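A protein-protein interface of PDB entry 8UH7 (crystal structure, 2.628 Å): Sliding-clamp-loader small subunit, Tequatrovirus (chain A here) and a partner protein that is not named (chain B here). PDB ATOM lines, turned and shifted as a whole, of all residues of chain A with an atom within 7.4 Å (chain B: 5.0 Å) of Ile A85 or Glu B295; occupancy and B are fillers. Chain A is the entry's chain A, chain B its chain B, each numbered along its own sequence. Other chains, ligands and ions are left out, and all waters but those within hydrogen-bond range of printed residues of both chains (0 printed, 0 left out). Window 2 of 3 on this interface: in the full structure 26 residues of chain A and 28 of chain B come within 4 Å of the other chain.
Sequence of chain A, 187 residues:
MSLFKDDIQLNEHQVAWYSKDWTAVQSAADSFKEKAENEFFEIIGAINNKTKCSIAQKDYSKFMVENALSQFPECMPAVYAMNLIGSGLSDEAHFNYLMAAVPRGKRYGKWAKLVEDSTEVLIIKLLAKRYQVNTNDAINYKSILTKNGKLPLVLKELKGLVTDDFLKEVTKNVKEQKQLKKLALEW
Of the 12 printed residues of chain A, 5 touch a printed residue of chain B.
Printed residues of chain A that touch a printed residue of chain B: Leu A84, Ile A85, Ser A87, Gly A88 and Tyr A97.
Hydrophobic or aromatic side chains of chain A that line the printed part of chain B: Ile A85 and Tyr A97.
Of the 10 printed residues of chain B, 6 touch a printed residue of chain A.
Among the printed residues, no Asp or Glu carboxylate lies within 4 Å of a Lys or Arg side-chain nitrogen of the other chain.
Tyr B290 touches Ile A85 (O to CD1, 3.8 Å).
Ile A85 touches Glu B291 (CD1 to O, 3.4 Å).
Ile A85 touches Glu B295 (CB to N, 3.5 Å).
Tyr A97 touches Tyr B290 (CD1 to CB, 3.6 Å).
The backbone carbonyl oxygen (O) of Leu A84 is in hydrogen-bond range of the side-chain amide nitrogen (NE2) of Gln B298 (2.9 Å).
NE2 of Gln B298 sits at hydrogen-bond distance from OG of Ser A87, 2.4 Å away.
OD1 of Asn B297 lies close to O of Gly A88, at 3.4 Å.
OH of Tyr A97 is in hydrogen-bond range of OE2 of Glu B291, 2.6 Å away.
The backbone carbonyl oxygen (O) of Ile A85 sits close to the backbone carbonyl oxygen (O) of Gly B294.
Ile A85 touches just these residues of chain B: Tyr B290, Glu B291, Gly B294 and Glu B295.
Glu B295 touches just one residue of chain A: Ile A85 (3.5 Å).
Of the printed residues of chain A, Gly B294 touches Ile A85 (3.0 Å).
Of the printed residues of chain B, Gly A88 touches Asn B297 (3.4 Å).
Printed residues of chain A within 4 Å of Glu B291: Ile A85 and Tyr A97.
Val A79 touches none of the printed residues of chain B.
The nearest printed residue of chain A that does not touch Glu B291 is Ala A81 (4.3 Å).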
ATOM      1  N   VAL A  79     -22.194  11.780  13.354  1.00  0.00           N
ATOM      2  CA  VAL A  79     -21.600  10.451  13.470  1.00  0.00           C
ATOM      3  C   VAL A  79     -20.189  10.452  12.903  1.00  0.00           C
ATOM      4  O   VAL A  79     -19.279   9.836  13.463  1.00  0.00           O
ATOM      5  CB  VAL A  79     -22.493   9.406  12.780  1.00  0.00           C
ATOM      6  CG1 VAL A  79     -21.852   8.029  12.838  1.00  0.00           C
ATOM      7  CG2 VAL A  79     -23.856   9.380  13.433  1.00  0.00           C
ATOM      8  N   TYR A  80     -19.982  11.156  11.791  1.00  0.00           N
ATOM      9  CA  TYR A  80     -18.650  11.278  11.209  1.00  0.00           C
ATOM     10  C   TYR A  80     -17.692  11.958  12.182  1.00  0.00           C
ATOM     11  O   TYR A  80     -16.568  11.486  12.402  1.00  0.00           O
ATOM     12  CB  TYR A  80     -18.758  12.050   9.892  1.00  0.00           C
ATOM     13  CG  TYR A  80     -17.461  12.371   9.188  1.00  0.00           C
ATOM     14  CD1 TYR A  80     -16.828  11.432   8.383  1.00  0.00           C
ATOM     15  CD2 TYR A  80     -16.891  13.632   9.294  1.00  0.00           C
ATOM     16  CE1 TYR A  80     -15.650  11.737   7.723  1.00  0.00           C
ATOM     17  CE2 TYR A  80     -15.718  13.944   8.642  1.00  0.00           C
ATOM     18  CZ  TYR A  80     -15.099  12.996   7.858  1.00  0.00           C
ATOM     19  OH  TYR A  80     -13.927  13.320   7.210  1.00  0.00           O
ATOM     20  N   ALA A  81     -18.134  13.059  12.795  1.00  0.00           N
ATOM     21  CA  ALA A  81     -17.277  13.777  13.735  1.00  0.00           C
ATOM     22  C   ALA A  81     -16.918  12.908  14.931  1.00  0.00           C
ATOM     23  O   ALA A  81     -15.756  12.873  15.354  1.00  0.00           O
ATOM     24  CB  ALA A  81     -17.960  15.062  14.196  1.00  0.00           C
ATOM     25  N   MET A  82     -17.899  12.195  15.490  1.00  0.00           N
ATOM     26  CA  MET A  82     -17.617  11.329  16.630  1.00  0.00           C
ATOM     27  C   MET A  82     -16.808  10.102  16.240  1.00  0.00           C
ATOM     28  O   MET A  82     -16.132   9.523  17.095  1.00  0.00           O
ATOM     29  CB  MET A  82     -18.919  10.906  17.304  1.00  0.00           C
ATOM     30  CG  MET A  82     -19.532  11.982  18.189  1.00  0.00           C
ATOM     31  SD  MET A  82     -18.501  12.409  19.611  1.00  0.00           S
ATOM     32  CE  MET A  82     -17.690  13.906  19.056  1.00  0.00           C
ATOM     33  N   ASN A  83     -16.868   9.693  14.974  1.00  0.00           N
ATOM     34  CA  ASN A  83     -16.063   8.581  14.492  1.00  0.00           C
ATOM     35  C   ASN A  83     -14.618   9.001  14.277  1.00  0.00           C
ATOM     36  O   ASN A  83     -13.709   8.173  14.405  1.00  0.00           O
ATOM     37  CB  ASN A  83     -16.684   8.037  13.201  1.00  0.00           C
ATOM     38  CG  ASN A  83     -15.903   6.889  12.603  1.00  0.00           C
ATOM     39  OD1 ASN A  83     -15.804   5.811  13.190  1.00  0.00           O
ATOM     40  ND2 ASN A  83     -15.368   7.103  11.406  1.00  0.00           N
ATOM     41  N   LEU A  84     -14.385  10.278  13.971  1.00  0.00           N
ATOM     42  CA  LEU A  84     -13.016  10.767  13.809  1.00  0.00           C
ATOM     43  C   LEU A  84     -12.379  11.115  15.153  1.00  0.00           C
ATOM     44  O   LEU A  84     -11.414  10.476  15.581  1.00  0.00           O
ATOM     45  CB  LEU A  84     -12.999  11.980  12.875  1.00  0.00           C
ATOM     46  CG  LEU A  84     -13.299  11.724  11.403  1.00  0.00           C
ATOM     47  CD1 LEU A  84     -12.993  12.969  10.605  1.00  0.00           C
ATOM     48  CD2 LEU A  84     -12.495  10.543  10.894  1.00  0.00           C
ATOM     49  N   ILE A  85     -12.915  12.131  15.833  1.00  0.00           N
ATOM     50  CA  ILE A  85     -12.270  12.681  17.023  1.00  0.00           C
ATOM     51  C   ILE A  85     -12.905  12.214  18.326  1.00  0.00           C
ATOM     52  O   ILE A  85     -12.368  12.521  19.403  1.00  0.00           O
ATOM     53  CB  ILE A  85     -12.260  14.224  16.978  1.00  0.00           C
ATOM     54  CG1 ILE A  85     -13.684  14.772  16.865  1.00  0.00           C
ATOM     55  CG2 ILE A  85     -11.414  14.714  15.814  1.00  0.00           C
ATOM     56  CD1 ILE A  85     -14.313  15.150  18.188  1.00  0.00           C
ATOM     57  N   GLY A  86     -14.021  11.499  18.272  1.00  0.00           N
ATOM     58  CA  GLY A  86     -14.714  11.116  19.483  1.00  0.00           C
ATOM     59  C   GLY A  86     -14.349   9.773  20.063  1.00  0.00           C
ATOM     60  O   GLY A  86     -14.917   9.385  21.091  1.00  0.00           O
ATOM     61  N   SER A  87     -13.417   9.044  19.443  1.00  0.00           N
ATOM     62  CA  SER A  87     -13.067   7.715  19.936  1.00  0.00           C
ATOM     63  C   SER A  87     -12.497   7.763  21.349  1.00  0.00           C
ATOM     64  O   SER A  87     -12.746   6.853  22.149  1.00  0.00           O
ATOM     65  CB  SER A  87     -12.081   7.047  18.979  1.00  0.00           C
ATOM     66  OG  SER A  87     -11.000   7.909  18.669  1.00  0.00           O
ATOM     67  N   GLY A  88     -11.751   8.811  21.684  1.00  0.00           N
ATOM     68  CA  GLY A  88     -11.177   8.922  23.010  1.00  0.00           C
ATOM     69  C   GLY A  88     -12.026   9.709  23.989  1.00  0.00           C
ATOM     70  O   GLY A  88     -11.540  10.118  25.048  1.00  0.00           O
ATOM     71  N   LEU A  89     -13.292   9.931  23.652  1.00  0.00           N
ATOM     72  CA  LEU A  89     -14.200  10.652  24.530  1.00  0.00           C
ATOM     73  C   LEU A  89     -14.917   9.691  25.473  1.00  0.00           C
ATOM     74  O   LEU A  89     -14.958   8.477  25.259  1.00  0.00           O
ATOM     75  CB  LEU A  89     -15.231  11.446  23.724  1.00  0.00           C
ATOM     76  CG  LEU A  89     -14.854  12.851  23.252  1.00  0.00           C
ATOM     77  CD1 LEU A  89     -16.023  13.501  22.528  1.00  0.00           C
ATOM     78  CD2 LEU A  89     -14.406  13.711  24.420  1.00  0.00           C
ATOM     79  N   TYR A  97     -22.545  15.214  23.257  1.00  0.00           N
ATOM     80  CA  TYR A  97     -22.288  15.814  21.955  1.00  0.00           C
ATOM     81  C   TYR A  97     -23.353  15.410  20.949  1.00  0.00           C
ATOM     82  O   TYR A  97     -23.838  16.248  20.182  1.00  0.00           O
ATOM     83  CB  TYR A  97     -20.907  15.420  21.438  1.00  0.00           C
ATOM     84  CG  TYR A  97     -20.682  15.876  20.015  1.00  0.00           C
ATOM     85  CD1 TYR A  97     -20.216  17.152  19.746  1.00  0.00           C
ATOM     86  CD2 TYR A  97     -20.956  15.039  18.939  1.00  0.00           C
ATOM     87  CE1 TYR A  97     -20.017  17.581  18.452  1.00  0.00           C
ATOM     88  CE2 TYR A  97     -20.763  15.461  17.637  1.00  0.00           C
ATOM     89  CZ  TYR A  97     -20.290  16.734  17.400  1.00  0.00           C
ATOM     90  OH  TYR A  97     -20.088  17.170  16.113  1.00  0.00           O
ATOM     91  N   TYR B 290     -16.844  19.824  22.650  1.00  0.00           N
ATOM     92  CA  TYR B 290     -16.622  18.388  22.543  1.00  0.00           C
ATOM     93  C   TYR B 290     -15.795  18.052  21.311  1.00  0.00           C
ATOM     94  O   TYR B 290     -14.924  17.181  21.372  1.00  0.00           O
ATOM     95  CB  TYR B 290     -17.954  17.643  22.542  1.00  0.00           C
ATOM     96  CG  TYR B 290     -18.494  17.428  23.935  1.00  0.00           C
ATOM     97  CD1 TYR B 290     -17.681  16.919  24.941  1.00  0.00           C
ATOM     98  CD2 TYR B 290     -19.804  17.753  24.252  1.00  0.00           C
ATOM     99  CE1 TYR B 290     -18.164  16.727  26.219  1.00  0.00           C
ATOM    100  CE2 TYR B 290     -20.296  17.564  25.529  1.00  0.00           C
ATOM    101  CZ  TYR B 290     -19.472  17.050  26.510  1.00  0.00           C
ATOM    102  OH  TYR B 290     -19.957  16.860  27.784  1.00  0.00           O
ATOM    103  N   GLU B 291     -16.011  18.759  20.199  1.00  0.00           N
ATOM    104  CA  GLU B 291     -15.186  18.511  19.018  1.00  0.00           C
ATOM    105  C   GLU B 291     -13.722  18.855  19.285  1.00  0.00           C
ATOM    106  O   GLU B 291     -12.816  18.065  18.975  1.00  0.00           O
ATOM    107  CB  GLU B 291     -15.726  19.300  17.825  1.00  0.00           C
ATOM    108  CG  GLU B 291     -17.001  18.715  17.238  1.00  0.00           C
ATOM    109  CD  GLU B 291     -17.633  19.608  16.190  1.00  0.00           C
ATOM    110  OE1 GLU B 291     -17.280  20.806  16.130  1.00  0.00           O
ATOM    111  OE2 GLU B 291     -18.483  19.112  15.421  1.00  0.00           O
ATOM    112  N   ILE B 292     -13.476  20.025  19.883  1.00  0.00           N
ATOM    113  CA  ILE B 292     -12.111  20.478  20.156  1.00  0.00           C
ATOM    114  C   ILE B 292     -11.408  19.515  21.103  1.00  0.00           C
ATOM    115  O   ILE B 292     -10.264  19.101  20.867  1.00  0.00           O
ATOM    116  CB  ILE B 292     -12.130  21.903  20.732  1.00  0.00           C
ATOM    117  CG1 ILE B 292     -12.554  22.913  19.668  1.00  0.00           C
ATOM    118  CG2 ILE B 292     -10.777  22.261  21.321  1.00  0.00           C
ATOM    119  CD1 ILE B 292     -12.766  24.303  20.220  1.00  0.00           C
ATOM    120  N   VAL B 293     -12.081  19.158  22.199  1.00  0.00           N
ATOM    121  CA  VAL B 293     -11.488  18.279  23.199  1.00  0.00           C
ATOM    122  C   VAL B 293     -11.250  16.892  22.619  1.00  0.00           C
ATOM    123  O   VAL B 293     -10.203  16.279  22.861  1.00  0.00           O
ATOM    124  CB  VAL B 293     -12.384  18.232  24.446  1.00  0.00           C
ATOM    125  CG1 VAL B 293     -12.004  17.067  25.330  1.00  0.00           C
ATOM    126  CG2 VAL B 293     -12.288  19.543  25.211  1.00  0.00           C
ATOM    127  N   GLY B 294     -12.206  16.375  21.845  1.00  0.00           N
ATOM    128  CA  GLY B 294     -12.016  15.079  21.226  1.00  0.00           C
ATOM    129  C   GLY B 294     -10.818  15.052  20.300  1.00  0.00           C
ATOM    130  O   GLY B 294     -10.024  14.111  20.332  1.00  0.00           O
ATOM    131  N   GLU B 295     -10.657  16.091  19.477  1.00  0.00           N
ATOM    132  CA  GLU B 295      -9.501  16.140  18.585  1.00  0.00           C
ATOM    133  C   GLU B 295      -8.200  16.216  19.379  1.00  0.00           C
ATOM    134  O   GLU B 295      -7.250  15.461  19.120  1.00  0.00           O
ATOM    135  CB  GLU B 295      -9.628  17.328  17.632  1.00  0.00           C
ATOM    136  CG  GLU B 295      -8.409  17.559  16.751  1.00  0.00           C
ATOM    137  CD  GLU B 295      -8.621  18.672  15.740  1.00  0.00           C
ATOM    138  OE1 GLU B 295      -9.777  18.876  15.312  1.00  0.00           O
ATOM    139  OE2 GLU B 295      -7.632  19.345  15.377  1.00  0.00           O
ATOM    140  N   ASN B 296      -8.148  17.118  20.364  1.00  0.00           N
ATOM    141  CA  ASN B 296      -6.925  17.308  21.136  1.00  0.00           C
ATOM    142  C   ASN B 296      -6.534  16.034  21.877  1.00  0.00           C
ATOM    143  O   ASN B 296      -5.347  15.709  21.984  1.00  0.00           O
ATOM    144  CB  ASN B 296      -7.108  18.473  22.110  1.00  0.00           C
ATOM    145  CG  ASN B 296      -5.836  18.822  22.853  1.00  0.00           C
ATOM    146  OD1 ASN B 296      -5.618  18.370  23.974  1.00  0.00           O
ATOM    147  ND2 ASN B 296      -4.992  19.637  22.235  1.00  0.00           N
ATOM    148  N   ASN B 297      -7.518  15.289  22.381  1.00  0.00           N
ATOM    149  CA  ASN B 297      -7.218  14.034  23.056  1.00  0.00           C
ATOM    150  C   ASN B 297      -6.868  12.929  22.066  1.00  0.00           C
ATOM    151  O   ASN B 297      -6.048  12.060  22.380  1.00  0.00           O
ATOM    152  CB  ASN B 297      -8.402  13.615  23.932  1.00  0.00           C
ATOM    153  CG  ASN B 297      -8.104  12.387  24.769  1.00  0.00           C
ATOM    154  OD1 ASN B 297      -8.390  11.261  24.361  1.00  0.00           O
ATOM    155  ND2 ASN B 297      -7.529  12.598  25.949  1.00  0.00           N
ATOM    156  N   GLN B 298      -7.468  12.948  20.872  1.00  0.00           N
ATOM    157  CA  GLN B 298      -7.143  11.953  19.859  1.00  0.00           C
ATOM    158  C   GLN B 298      -5.696  12.081  19.411  1.00  0.00           C
ATOM    159  O   GLN B 298      -5.035  11.077  19.115  1.00  0.00           O
ATOM    160  CB  GLN B 298      -8.090  12.095  18.666  1.00  0.00           C
ATOM    161  CG  GLN B 298      -7.770  11.183  17.495  1.00  0.00           C
ATOM    162  CD  GLN B 298      -8.299   9.775  17.677  1.00  0.00           C
ATOM    163  OE1 GLN B 298      -7.531   8.817  17.758  1.00  0.00           O
ATOM    164  NE2 GLN B 298      -9.619   9.642  17.733  1.00  0.00           N
ATOM    165  N   TYR B 299      -5.178  13.308  19.354  1.00  0.00           N
ATOM    166  CA  TYR B 299      -3.775  13.512  19.017  1.00  0.00           C
ATOM    167  C   TYR B 299      -2.882  13.619  20.246  1.00  0.00           C
ATOM    168  O   TYR B 299      -1.887  14.355  20.220  1.00  0.00           O
ATOM    169  CB  TYR B 299      -3.616  14.751  18.142  1.00  0.00           C
ATOM    170  CG  TYR B 299      -4.232  14.618  16.774  1.00  0.00           C
ATOM    171  CD1 TYR B 299      -3.537  14.014  15.737  1.00  0.00           C
ATOM    172  CD2 TYR B 299      -5.506  15.102  16.518  1.00  0.00           C
ATOM    173  CE1 TYR B 299      -4.096  13.893  14.484  1.00  0.00           C
ATOM    174  CE2 TYR B 299      -6.073  14.986  15.269  1.00  0.00           C
ATOM    175  CZ  TYR B 299      -5.363  14.382  14.255  1.00  0.00           C
ATOM    176  OH  TYR B 299      -5.927  14.268  13.010  1.00  0.00           O
